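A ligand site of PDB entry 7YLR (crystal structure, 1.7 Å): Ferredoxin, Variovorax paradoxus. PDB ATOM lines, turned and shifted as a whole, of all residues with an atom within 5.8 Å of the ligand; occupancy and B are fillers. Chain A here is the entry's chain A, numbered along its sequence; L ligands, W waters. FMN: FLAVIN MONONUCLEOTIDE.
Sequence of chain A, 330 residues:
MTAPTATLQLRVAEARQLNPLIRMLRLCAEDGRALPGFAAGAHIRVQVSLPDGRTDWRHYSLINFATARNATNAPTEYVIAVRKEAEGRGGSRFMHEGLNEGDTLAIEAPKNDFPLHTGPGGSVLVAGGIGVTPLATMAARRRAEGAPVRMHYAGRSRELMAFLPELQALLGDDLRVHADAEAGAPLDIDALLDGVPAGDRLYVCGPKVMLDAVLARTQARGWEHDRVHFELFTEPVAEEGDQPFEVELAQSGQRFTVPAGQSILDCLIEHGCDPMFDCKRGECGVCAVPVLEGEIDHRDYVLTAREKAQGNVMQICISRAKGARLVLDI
The side-chain hydroxyl (OG) of Ser 92 sits close to the backbone carbonyl oxygen (O) of Arg 83 (3.5 Å). N of Glu 85 sits at hydrogen-bond distance from OG of Ser 92 (2.9 Å). The backbone carbonyl oxygen (O) of Ile 130 lies within hydrogen-bond range of the side-chain hydroxyl (OG1) of Thr 133, 3.2 Å away. OE1 of Glu 235 lies within salt-bridge range of NH2 of Arg 89. The side-chain carboxylate of Glu 85 lies within salt-bridge range of the guanidinium group of Arg 83 (3.1 Å). The guanidinium group (NH2) of Arg 281 lies within salt-bridge range of the side-chain carboxylate (OE1) of Glu 231 (2.8 Å). The guanidinium group of Arg 281 lies within salt-bridge range of the side-chain carboxylate of Asp 113 (2.9 Å). O of Gly 88 lies within hydrogen-bond range of NH1 of Arg 93 (3.1 Å).
Merely in contact with the ligand: Phe 233 (3.1 Å), Arg 281 (3.4 Å), Gly 88 (3.6 Å), Leu 232 (3.6 Å), Val 82 (3.6 Å), Gly 90 (3.6 Å), Ile 130 (3.7 Å), Glu 231 (3.7 Å) and His 43 (3.9 Å). Hydrophobic or aromatic side chains that line the ligand: His 59, Tyr 60, Ile 130 and Phe 233. The nearest printed residue that does not touch the ligand is Glu 85 (4.1 Å).
An oxygen (O2') of the ligand lies within hydrogen-bond range of the backbone NH of His 59, at 3.4 Å. An oxygen (O2') of the ligand lies within hydrogen-bond range of the backbone carbonyl oxygen (O) of His 59 (2.6 Å). The backbone NH (N) of Ser 92 lies within hydrogen-bond range of an oxygen (O1P) of the ligand, at 2.9 Å. OG of Ser 92 sits at hydrogen-bond distance from O1P of the ligand, at 2.7 Å. The backbone NH (N) of Gly 91 sits at hydrogen-bond distance from an oxygen (O3P) of the ligand (2.8 Å). OG1 of Thr 133 is in hydrogen-bond range of O4 of the ligand (2.8 Å). The backbone NH (N) of Arg 89 sits at hydrogen-bond distance from an oxygen (O2P) of the ligand, 2.8 Å away. The guanidinium group of Arg 89 lies within salt-bridge range of an oxygen (O2P) of the ligand, at 3.0 Å. NE of Arg 58 is in salt-bridge range of O3P of the ligand, 2.8 Å away. N of Arg 83 sits at hydrogen-bond distance from O2 of the ligand (2.9 Å). The backbone carbonyl oxygen (O) of Ala 81 lies within hydrogen-bond range of a nitrogen (N3) of the ligand (2.9 Å). O4' of the ligand is in hydrogen-bond range of OH of Tyr 60. The side-chain carboxylate (OE1) of Glu 235 is in hydrogen-bond range of an oxygen (O3') of the ligand (3.0 Å). The backbone NH of Ser 61 sits at hydrogen-bond distance from an oxygen (O4) of the ligand (3.2 Å). The side-chain hydroxyl (OG) of Ser 61 is in hydrogen-bond range of a nitrogen (N5) of the ligand.
Water W6 lies within hydrogen-bond range of O1P of the ligand (2.5 Å), N of Gly 90 (2.8 Å), O of Glu 85 (3.0 Å), OG of Ser 92 (3.2 Å) and N of Arg 93 (3.3 Å). Water W2 lies within hydrogen-bond range of O4' of the ligand and O of Arg 83. Water W5 lies within hydrogen-bond range of O4 of the ligand (2.6 Å), O of Ser 61 (2.7 Å) and N of Ala 81 (2.8 Å). Water W3 lies within hydrogen-bond range of O3' of the ligand (2.7 Å), O of Phe 233 (3.0 Å) and N of Glu 235 (3.1 Å). Water W4 lies within hydrogen-bond range of the side-chain carboxylate of Glu 235 (2.6 Å), a ring nitrogen (ND1) of His 59 (2.8 Å) and an oxygen (O2') of the ligand (3.0 Å).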
ATOM      1  N   HIS A  43      -3.907 -32.413 -16.362  1.00  0.00           N
ATOM      2  CA  HIS A  43      -2.476 -32.487 -16.094  1.00  0.00           C
ATOM      3  C   HIS A  43      -2.021 -33.927 -16.253  1.00  0.00           C
ATOM      4  O   HIS A  43      -2.848 -34.859 -16.293  1.00  0.00           O
ATOM      5  CB  HIS A  43      -2.142 -32.000 -14.674  1.00  0.00           C
ATOM      6  CG  HIS A  43      -2.756 -32.849 -13.619  1.00  0.00           C
ATOM      7  ND1 HIS A  43      -4.015 -32.605 -13.102  1.00  0.00           N
ATOM      8  CD2 HIS A  43      -2.319 -33.989 -13.028  1.00  0.00           C
ATOM      9  CE1 HIS A  43      -4.317 -33.538 -12.212  1.00  0.00           C
ATOM     10  NE2 HIS A  43      -3.303 -34.386 -12.139  1.00  0.00           N
ATOM     11  N   LEU A  50      14.673 -37.475  -7.355  1.00  0.00           N
ATOM     12  CA  LEU A  50      15.024 -36.448  -6.383  1.00  0.00           C
ATOM     13  C   LEU A  50      16.530 -36.450  -6.136  1.00  0.00           C
ATOM     14  O   LEU A  50      17.261 -37.310  -6.636  1.00  0.00           O
ATOM     15  CB  LEU A  50      14.220 -36.677  -5.107  1.00  0.00           C
ATOM     16  CG  LEU A  50      12.707 -36.671  -5.301  1.00  0.00           C
ATOM     17  CD1 LEU A  50      11.998 -36.925  -3.967  1.00  0.00           C
ATOM     18  CD2 LEU A  50      12.253 -35.371  -5.941  1.00  0.00           C
ATOM     19  N   ARG A  58       5.518 -35.696 -10.108  1.00  0.00           N
ATOM     20  CA  ARG A  58       5.247 -34.265 -10.164  1.00  0.00           C
ATOM     21  C   ARG A  58       4.132 -33.996 -11.176  1.00  0.00           C
ATOM     22  O   ARG A  58       4.156 -34.509 -12.294  1.00  0.00           O
ATOM     23  CB  ARG A  58       6.512 -33.472 -10.571  1.00  0.00           C
ATOM     24  CG  ARG A  58       7.586 -33.399  -9.471  1.00  0.00           C
ATOM     25  CD  ARG A  58       7.060 -32.757  -8.215  1.00  0.00           C
ATOM     26  NE  ARG A  58       8.083 -32.645  -7.181  1.00  0.00           N
ATOM     27  CZ  ARG A  58       8.237 -33.510  -6.190  1.00  0.00           C
ATOM     28  NH1 ARG A  58       7.501 -34.603  -6.085  1.00  0.00           N
ATOM     29  NH2 ARG A  58       9.165 -33.265  -5.257  1.00  0.00           N
ATOM     30  N   HIS A  59       3.165 -33.163 -10.778  1.00  0.00           N
ATOM     31  CA  HIS A  59       2.110 -32.748 -11.697  1.00  0.00           C
ATOM     32  C   HIS A  59       2.617 -31.655 -12.622  1.00  0.00           C
ATOM     33  O   HIS A  59       3.210 -30.677 -12.161  1.00  0.00           O
ATOM     34  CB  HIS A  59       0.893 -32.153 -10.979  1.00  0.00           C
ATOM     35  CG  HIS A  59       0.294 -33.010  -9.909  1.00  0.00           C
ATOM     36  ND1 HIS A  59       0.863 -33.147  -8.656  1.00  0.00           N
ATOM     37  CD2 HIS A  59      -0.910 -33.626  -9.842  1.00  0.00           C
ATOM     38  CE1 HIS A  59       0.080 -33.911  -7.905  1.00  0.00           C
ATOM     39  NE2 HIS A  59      -1.009 -34.190  -8.597  1.00  0.00           N
ATOM     40  N   TYR A  60       2.315 -31.779 -13.933  1.00  0.00           N
ATOM     41  CA  TYR A  60       2.513 -30.692 -14.896  1.00  0.00           C
ATOM     42  C   TYR A  60       1.307 -30.605 -15.829  1.00  0.00           C
ATOM     43  O   TYR A  60       0.827 -31.619 -16.354  1.00  0.00           O
ATOM     44  CB  TYR A  60       3.849 -30.839 -15.697  1.00  0.00           C
ATOM     45  CG  TYR A  60       5.018 -30.700 -14.755  1.00  0.00           C
ATOM     46  CD1 TYR A  60       5.273 -29.489 -14.123  1.00  0.00           C
ATOM     47  CD2 TYR A  60       5.818 -31.791 -14.437  1.00  0.00           C
ATOM     48  CE1 TYR A  60       6.293 -29.372 -13.185  1.00  0.00           C
ATOM     49  CE2 TYR A  60       6.831 -31.684 -13.518  1.00  0.00           C
ATOM     50  CZ  TYR A  60       7.063 -30.471 -12.894  1.00  0.00           C
ATOM     51  OH  TYR A  60       8.079 -30.386 -11.975  1.00  0.00           O
ATOM     52  N   SER A  61       0.797 -29.386 -16.006  1.00  0.00           N
ATOM     53  CA  SER A  61      -0.419 -29.185 -16.794  1.00  0.00           C
ATOM     54  C   SER A  61      -0.139 -29.341 -18.294  1.00  0.00           C
ATOM     55  O   SER A  61       0.933 -28.972 -18.788  1.00  0.00           O
ATOM     56  CB  SER A  61      -0.962 -27.773 -16.545  1.00  0.00           C
ATOM     57  OG  SER A  61      -1.373 -27.613 -15.210  1.00  0.00           O
ATOM     58  N   ILE A  80       4.386 -29.873 -21.878  1.00  0.00           N
ATOM     59  CA  ILE A  80       4.381 -29.286 -20.545  1.00  0.00           C
ATOM     60  C   ILE A  80       5.476 -28.232 -20.496  1.00  0.00           C
ATOM     61  O   ILE A  80       6.364 -28.171 -21.351  1.00  0.00           O
ATOM     62  CB  ILE A  80       4.578 -30.363 -19.445  1.00  0.00           C
ATOM     63  CG1 ILE A  80       5.927 -31.070 -19.645  1.00  0.00           C
ATOM     64  CG2 ILE A  80       3.474 -31.399 -19.526  1.00  0.00           C
ATOM     65  CD1 ILE A  80       6.370 -31.974 -18.475  1.00  0.00           C
ATOM     66  N   ALA A  81       5.405 -27.373 -19.469  1.00  0.00           N
ATOM     67  CA  ALA A  81       6.407 -26.340 -19.254  1.00  0.00           C
ATOM     68  C   ALA A  81       6.685 -26.238 -17.764  1.00  0.00           C
ATOM     69  O   ALA A  81       5.753 -26.043 -16.971  1.00  0.00           O
ATOM     70  CB  ALA A  81       5.940 -24.992 -19.803  1.00  0.00           C
ATOM     71  N   VAL A  82       7.957 -26.386 -17.389  1.00  0.00           N
ATOM     72  CA  VAL A  82       8.382 -26.572 -16.005  1.00  0.00           C
ATOM     73  C   VAL A  82       9.200 -25.369 -15.562  1.00  0.00           C
ATOM     74  O   VAL A  82      10.237 -25.053 -16.175  1.00  0.00           O
ATOM     75  CB  VAL A  82       9.198 -27.859 -15.830  1.00  0.00           C
ATOM     76  CG1 VAL A  82       9.654 -28.024 -14.384  1.00  0.00           C
ATOM     77  CG2 VAL A  82       8.419 -29.080 -16.299  1.00  0.00           C
ATOM     78  N   ARG A  83       8.777 -24.723 -14.478  1.00  0.00           N
ATOM     79  CA  ARG A  83       9.561 -23.651 -13.866  1.00  0.00           C
ATOM     80  C   ARG A  83      10.585 -24.273 -12.909  1.00  0.00           C
ATOM     81  O   ARG A  83      10.206 -24.998 -11.981  1.00  0.00           O
ATOM     82  CB  ARG A  83       8.654 -22.678 -13.128  1.00  0.00           C
ATOM     83  CG  ARG A  83       9.394 -21.535 -12.441  1.00  0.00           C
ATOM     84  CD  ARG A  83       8.441 -20.671 -11.625  1.00  0.00           C
ATOM     85  NE  ARG A  83       9.201 -19.738 -10.800  1.00  0.00           N
ATOM     86  CZ  ARG A  83       9.418 -18.467 -11.104  1.00  0.00           C
ATOM     87  NH1 ARG A  83       8.877 -17.909 -12.178  1.00  0.00           N
ATOM     88  NH2 ARG A  83      10.203 -17.734 -10.318  1.00  0.00           N
ATOM     89  N   LYS A  84      11.866 -23.997 -13.151  1.00  0.00           N
ATOM     90  CA  LYS A  84      12.916 -24.530 -12.281  1.00  0.00           C
ATOM     91  C   LYS A  84      12.883 -23.847 -10.924  1.00  0.00           C
ATOM     92  O   LYS A  84      12.924 -22.618 -10.841  1.00  0.00           O
ATOM     93  CB  LYS A  84      14.277 -24.319 -12.931  1.00  0.00           C
ATOM     94  CG  LYS A  84      15.392 -25.023 -12.155  1.00  0.00           C
ATOM     95  CD  LYS A  84      16.770 -24.595 -12.674  1.00  0.00           C
ATOM     96  CE  LYS A  84      17.801 -25.663 -12.362  1.00  0.00           C
ATOM     97  NZ  LYS A  84      19.036 -25.543 -13.211  1.00  0.00           N
ATOM     98  N   GLU A  85      12.812 -24.650  -9.851  1.00  0.00           N
ATOM     99  CA  GLU A  85      12.833 -24.118  -8.484  1.00  0.00           C
ATOM    100  C   GLU A  85      14.162 -24.526  -7.858  1.00  0.00           C
ATOM    101  O   GLU A  85      14.318 -25.650  -7.364  1.00  0.00           O
ATOM    102  CB  GLU A  85      11.627 -24.609  -7.688  1.00  0.00           C
ATOM    103  CG  GLU A  85      10.285 -24.077  -8.241  1.00  0.00           C
ATOM    104  CD  GLU A  85      10.147 -22.549  -8.141  1.00  0.00           C
ATOM    105  OE1 GLU A  85      11.012 -21.886  -7.517  1.00  0.00           O
ATOM    106  OE2 GLU A  85       9.174 -22.000  -8.699  1.00  0.00           O
ATOM    107  N   GLY A  88      13.585 -25.658  -4.473  1.00  0.00           N
ATOM    108  CA  GLY A  88      12.527 -26.623  -4.285  1.00  0.00           C
ATOM    109  C   GLY A  88      13.053 -27.977  -3.839  1.00  0.00           C
ATOM    110  O   GLY A  88      14.203 -28.121  -3.426  1.00  0.00           O
ATOM    111  N   ARG A  89      12.181 -28.985  -3.939  1.00  0.00           N
ATOM    112  CA  ARG A  89      12.481 -30.330  -3.468  1.00  0.00           C
ATOM    113  C   ARG A  89      13.320 -31.157  -4.452  1.00  0.00           C
ATOM    114  O   ARG A  89      13.700 -32.285  -4.116  1.00  0.00           O
ATOM    115  CB  ARG A  89      11.182 -31.086  -3.163  1.00  0.00           C
ATOM    116  CG  ARG A  89      10.290 -30.382  -2.144  1.00  0.00           C
ATOM    117  CD  ARG A  89       8.869 -30.866  -2.278  1.00  0.00           C
ATOM    118  NE  ARG A  89       8.308 -30.476  -3.569  1.00  0.00           N
ATOM    119  CZ  ARG A  89       7.096 -30.848  -3.995  1.00  0.00           C
ATOM    120  NH1 ARG A  89       6.331 -31.650  -3.278  1.00  0.00           N
ATOM    121  NH2 ARG A  89       6.657 -30.403  -5.168  1.00  0.00           N
ATOM    122  N   GLY A  90      13.630 -30.619  -5.623  1.00  0.00           N
ATOM    123  CA  GLY A  90      14.470 -31.311  -6.582  1.00  0.00           C
ATOM    124  C   GLY A  90      13.731 -31.825  -7.798  1.00  0.00           C
ATOM    125  O   GLY A  90      14.395 -32.209  -8.766  1.00  0.00           O
ATOM    126  N   GLY A  91      12.409 -31.847  -7.793  1.00  0.00           N
ATOM    127  CA  GLY A  91      11.687 -32.400  -8.932  1.00  0.00           C
ATOM    128  C   GLY A  91      11.771 -31.528 -10.166  1.00  0.00           C
ATOM    129  O   GLY A  91      12.067 -32.013 -11.271  1.00  0.00           O
ATOM    130  N   SER A  92      11.494 -30.233 -10.023  1.00  0.00           N
ATOM    131  CA  SER A  92      11.646 -29.321 -11.149  1.00  0.00           C
ATOM    132  C   SER A  92      13.111 -29.167 -11.549  1.00  0.00           C
ATOM    133  O   SER A  92      13.411 -28.986 -12.733  1.00  0.00           O
ATOM    134  CB  SER A  92      11.001 -27.963 -10.836  1.00  0.00           C
ATOM    135  OG  SER A  92      11.687 -27.274  -9.817  1.00  0.00           O
ATOM    136  N   ARG A  93      14.035 -29.265 -10.587  1.00  0.00           N
ATOM    137  CA  ARG A  93      15.442 -29.271 -10.957  1.00  0.00           C
ATOM    138  C   ARG A  93      15.759 -30.467 -11.837  1.00  0.00           C
ATOM    139  O   ARG A  93      16.491 -30.334 -12.821  1.00  0.00           O
ATOM    140  CB  ARG A  93      16.363 -29.276  -9.730  1.00  0.00           C
ATOM    141  CG  ARG A  93      16.412 -28.009  -8.883  1.00  0.00           C
ATOM    142  CD  ARG A  93      17.737 -27.972  -8.056  1.00  0.00           C
ATOM    143  NE  ARG A  93      17.793 -28.944  -6.975  1.00  0.00           N
ATOM    144  CZ  ARG A  93      17.196 -28.801  -5.801  1.00  0.00           C
ATOM    145  NH1 ARG A  93      16.531 -27.702  -5.491  1.00  0.00           N
ATOM    146  NH2 ARG A  93      17.247 -29.795  -4.923  1.00  0.00           N
ATOM    147  N   ASP A 113      -8.687 -32.151 -12.786  1.00  0.00           N
ATOM    148  CA  ASP A 113      -9.386 -31.623 -11.620  1.00  0.00           C
ATOM    149  C   ASP A 113      -9.834 -30.185 -11.821  1.00  0.00           C
ATOM    150  O   ASP A 113     -10.311 -29.562 -10.869  1.00  0.00           O
ATOM    151  CB  ASP A 113      -8.480 -31.697 -10.389  1.00  0.00           C
ATOM    152  CG  ASP A 113      -7.970 -33.102 -10.112  1.00  0.00           C
ATOM    153  OD1 ASP A 113      -8.814 -34.005  -9.970  1.00  0.00           O
ATOM    154  OD2 ASP A 113      -6.737 -33.275  -9.989  1.00  0.00           O
ATOM    155  N   ILE A 130       3.748 -19.322 -13.896  1.00  0.00           N
ATOM    156  CA  ILE A 130       3.656 -20.554 -14.666  1.00  0.00           C
ATOM    157  C   ILE A 130       2.276 -21.210 -14.558  1.00  0.00           C
ATOM    158  O   ILE A 130       1.990 -22.168 -15.298  1.00  0.00           O
ATOM    159  CB  ILE A 130       4.807 -21.504 -14.252  1.00  0.00           C
ATOM    160  CG1 ILE A 130       5.055 -22.599 -15.312  1.00  0.00           C
ATOM    161  CG2 ILE A 130       4.590 -22.060 -12.863  1.00  0.00           C
ATOM    162  CD1 ILE A 130       5.295 -22.090 -16.738  1.00  0.00           C
ATOM    163  N   THR A 133      -0.136 -22.328 -17.598  1.00  0.00           N
ATOM    164  CA  THR A 133      -0.081 -23.483 -18.504  1.00  0.00           C
ATOM    165  C   THR A 133      -1.446 -24.126 -18.788  1.00  0.00           C
ATOM    166  O   THR A 133      -1.772 -24.280 -19.970  1.00  0.00           O
ATOM    167  CB  THR A 133       0.957 -24.519 -18.016  1.00  0.00           C
ATOM    168  OG1 THR A 133       0.756 -24.839 -16.632  1.00  0.00           O
ATOM    169  CG2 THR A 133       2.379 -23.984 -18.194  1.00  0.00           C
ATOM    170  N   PRO A 134      -2.303 -24.481 -17.808  1.00  0.00           N
ATOM    171  CA  PRO A 134      -3.600 -25.039 -18.208  1.00  0.00           C
ATOM    172  C   PRO A 134      -4.524 -23.984 -18.742  1.00  0.00           C
ATOM    173  O   PRO A 134      -5.403 -24.283 -19.570  1.00  0.00           O
ATOM    174  CB  PRO A 134      -4.157 -25.657 -16.917  1.00  0.00           C
ATOM    175  CG  PRO A 134      -3.582 -24.801 -15.869  1.00  0.00           C
ATOM    176  CD  PRO A 134      -2.189 -24.426 -16.346  1.00  0.00           C
ATOM    177  N   GLU A 231      -7.031 -23.901  -9.332  1.00  0.00           N
ATOM    178  CA  GLU A 231      -5.998 -24.907  -9.554  1.00  0.00           C
ATOM    179  C   GLU A 231      -4.722 -24.457  -8.848  1.00  0.00           C
ATOM    180  O   GLU A 231      -4.043 -23.531  -9.317  1.00  0.00           O
ATOM    181  CB  GLU A 231      -5.749 -25.117 -11.053  1.00  0.00           C
ATOM    182  CG  GLU A 231      -4.757 -26.253 -11.384  1.00  0.00           C
ATOM    183  CD  GLU A 231      -5.346 -27.662 -11.259  1.00  0.00           C
ATOM    184  OE1 GLU A 231      -5.817 -28.030 -10.160  1.00  0.00           O
ATOM    185  OE2 GLU A 231      -5.312 -28.409 -12.256  1.00  0.00           O
ATOM    186  N   LEU A 232      -4.384 -25.125  -7.745  1.00  0.00           N
ATOM    187  CA  LEU A 232      -3.280 -24.714  -6.878  1.00  0.00           C
ATOM    188  C   LEU A 232      -2.000 -25.442  -7.285  1.00  0.00           C
ATOM    189  O   LEU A 232      -1.933 -26.665  -7.162  1.00  0.00           O
ATOM    190  CB  LEU A 232      -3.626 -25.020  -5.417  1.00  0.00           C
ATOM    191  CG  LEU A 232      -2.517 -24.763  -4.393  1.00  0.00           C
ATOM    192  CD1 LEU A 232      -2.270 -23.266  -4.232  1.00  0.00           C
ATOM    193  CD2 LEU A 232      -2.854 -25.427  -3.057  1.00  0.00           C
ATOM    194  N   PHE A 233      -1.002 -24.690  -7.770  1.00  0.00           N
ATOM    195  CA  PHE A 233       0.279 -25.288  -8.139  1.00  0.00           C
ATOM    196  C   PHE A 233       1.207 -25.449  -6.929  1.00  0.00           C
ATOM    197  O   PHE A 233       2.031 -26.374  -6.912  1.00  0.00           O
ATOM    198  CB  PHE A 233       1.009 -24.448  -9.190  1.00  0.00           C
ATOM    199  CG  PHE A 233       0.561 -24.664 -10.612  1.00  0.00           C
ATOM    200  CD1 PHE A 233      -0.587 -25.385 -10.908  1.00  0.00           C
ATOM    201  CD2 PHE A 233       1.326 -24.149 -11.662  1.00  0.00           C
ATOM    202  CE1 PHE A 233      -0.966 -25.563 -12.222  1.00  0.00           C
ATOM    203  CE2 PHE A 233       0.962 -24.343 -12.972  1.00  0.00           C
ATOM    204  CZ  PHE A 233      -0.183 -25.041 -13.260  1.00  0.00           C
ATOM    205  N   THR A 234       1.086 -24.573  -5.930  1.00  0.00           N
ATOM    206  CA  THR A 234       2.058 -24.530  -4.841  1.00  0.00           C
ATOM    207  C   THR A 234       2.093 -25.846  -4.062  1.00  0.00           C
ATOM    208  O   THR A 234       1.075 -26.330  -3.560  1.00  0.00           O
ATOM    209  CB  THR A 234       1.751 -23.369  -3.905  1.00  0.00           C
ATOM    210  OG1 THR A 234       1.635 -22.172  -4.679  1.00  0.00           O
ATOM    211  CG2 THR A 234       2.885 -23.181  -2.881  1.00  0.00           C
ATOM    212  N   GLU A 235       3.299 -26.414  -3.975  1.00  0.00           N
ATOM    213  CA  GLU A 235       3.635 -27.630  -3.246  1.00  0.00           C
ATOM    214  C   GLU A 235       4.945 -27.433  -2.507  1.00  0.00           C
ATOM    215  O   GLU A 235       5.861 -26.771  -3.036  1.00  0.00           O
ATOM    216  CB  GLU A 235       3.765 -28.843  -4.175  1.00  0.00           C
ATOM    217  CG  GLU A 235       2.545 -29.196  -4.977  1.00  0.00           C
ATOM    218  CD  GLU A 235       2.697 -30.571  -5.578  1.00  0.00           C
ATOM    219  OE1 GLU A 235       3.853 -30.936  -5.889  1.00  0.00           O
ATOM    220  OE2 GLU A 235       1.693 -31.321  -5.679  1.00  0.00           O
ATOM    221  N   ARG A 281      -5.381 -31.409  -2.807  1.00  0.00           N
ATOM    222  CA  ARG A 281      -4.994 -30.008  -2.738  1.00  0.00           C
ATOM    223  C   ARG A 281      -6.198 -29.071  -2.597  1.00  0.00           C
ATOM    224  O   ARG A 281      -6.184 -27.950  -3.125  1.00  0.00           O
ATOM    225  CB  ARG A 281      -4.124 -29.632  -3.949  1.00  0.00           C
ATOM    226  CG  ARG A 281      -4.777 -29.973  -5.302  1.00  0.00           C
ATOM    227  CD  ARG A 281      -3.911 -29.417  -6.451  1.00  0.00           C
ATOM    228  NE  ARG A 281      -4.511 -29.585  -7.769  1.00  0.00           N
ATOM    229  CZ  ARG A 281      -4.720 -30.756  -8.376  1.00  0.00           C
ATOM    230  NH1 ARG A 281      -4.304 -31.889  -7.844  1.00  0.00           N
ATOM    231  NH2 ARG A 281      -5.317 -30.762  -9.561  1.00  0.00           N
HETATM  232  N1  FMN L   1       4.670 -26.513 -12.088  1.00  0.00           N
HETATM  233  C2  FMN L   1       5.179 -26.010 -13.251  1.00  0.00           C
HETATM  234  O2  FMN L   1       6.309 -25.496 -13.269  1.00  0.00           O
HETATM  235  N3  FMN L   1       4.425 -26.089 -14.405  1.00  0.00           N
HETATM  236  C4  FMN L   1       3.174 -26.643 -14.432  1.00  0.00           C
HETATM  237  O4  FMN L   1       2.522 -26.693 -15.501  1.00  0.00           O
HETATM  238  C4A FMN L   1       2.651 -27.162 -13.246  1.00  0.00           C
HETATM  239  N5  FMN L   1       1.399 -27.748 -13.209  1.00  0.00           N
HETATM  240  C5A FMN L   1       0.913 -28.250 -12.015  1.00  0.00           C
HETATM  241  C6  FMN L   1      -0.352 -28.811 -11.970  1.00  0.00           C
HETATM  242  C7  FMN L   1      -0.879 -29.316 -10.795  1.00  0.00           C
HETATM  243  C7M FMN L   1      -2.257 -29.936 -10.800  1.00  0.00           C
HETATM  244  C8  FMN L   1      -0.129 -29.256  -9.624  1.00  0.00           C
HETATM  245  C8M FMN L   1      -0.705 -29.809  -8.349  1.00  0.00           C
HETATM  246  C9  FMN L   1       1.145 -28.676  -9.639  1.00  0.00           C
HETATM  247  C9A FMN L   1       1.674 -28.161 -10.841  1.00  0.00           C
HETATM  248  N10 FMN L   1       2.925 -27.579 -10.902  1.00  0.00           N
HETATM  249  C10 FMN L   1       3.415 -27.091 -12.086  1.00  0.00           C
HETATM  250  C1' FMN L   1       3.827 -27.518  -9.691  1.00  0.00           C
HETATM  251  C2' FMN L   1       4.725 -28.794  -9.785  1.00  0.00           C
HETATM  252  O2' FMN L   1       3.994 -30.016  -9.747  1.00  0.00           O
HETATM  253  C3' FMN L   1       5.802 -28.905  -8.697  1.00  0.00           C
HETATM  254  O3' FMN L   1       5.241 -28.704  -7.418  1.00  0.00           O
HETATM  255  C4' FMN L   1       6.942 -27.903  -8.934  1.00  0.00           C
HETATM  256  O4' FMN L   1       7.610 -28.168 -10.160  1.00  0.00           O
HETATM  257  C5' FMN L   1       7.941 -27.903  -7.775  1.00  0.00           C
HETATM  258  O5' FMN L   1       8.432 -29.193  -7.443  1.00  0.00           O
HETATM  259  P   FMN L   1       9.871 -29.318  -6.734  1.00  0.00           P
HETATM  260  O1P FMN L   1      10.877 -28.644  -7.636  1.00  0.00           O
HETATM  261  O2P FMN L   1       9.784 -28.610  -5.401  1.00  0.00           O
HETATM  262  O3P FMN L   1      10.152 -30.790  -6.571  1.00  0.00           O
HETATM  263  O   HOH W   1       4.625 -23.977  -9.862  1.00  0.00           O
HETATM  264  O   HOH W   2       7.812 -25.757 -11.145  1.00  0.00           O
HETATM  265  O   HOH W   3       4.993 -26.171  -6.559  1.00  0.00           O
HETATM  266  O   HOH W   4       3.515 -32.348  -7.995  1.00  0.00           O
HETATM  267  O   HOH W   5       3.104 -27.588 -17.895  1.00  0.00           O
HETATM  268  O   HOH W   6      13.415 -28.500  -7.469  1.00  0.00           O
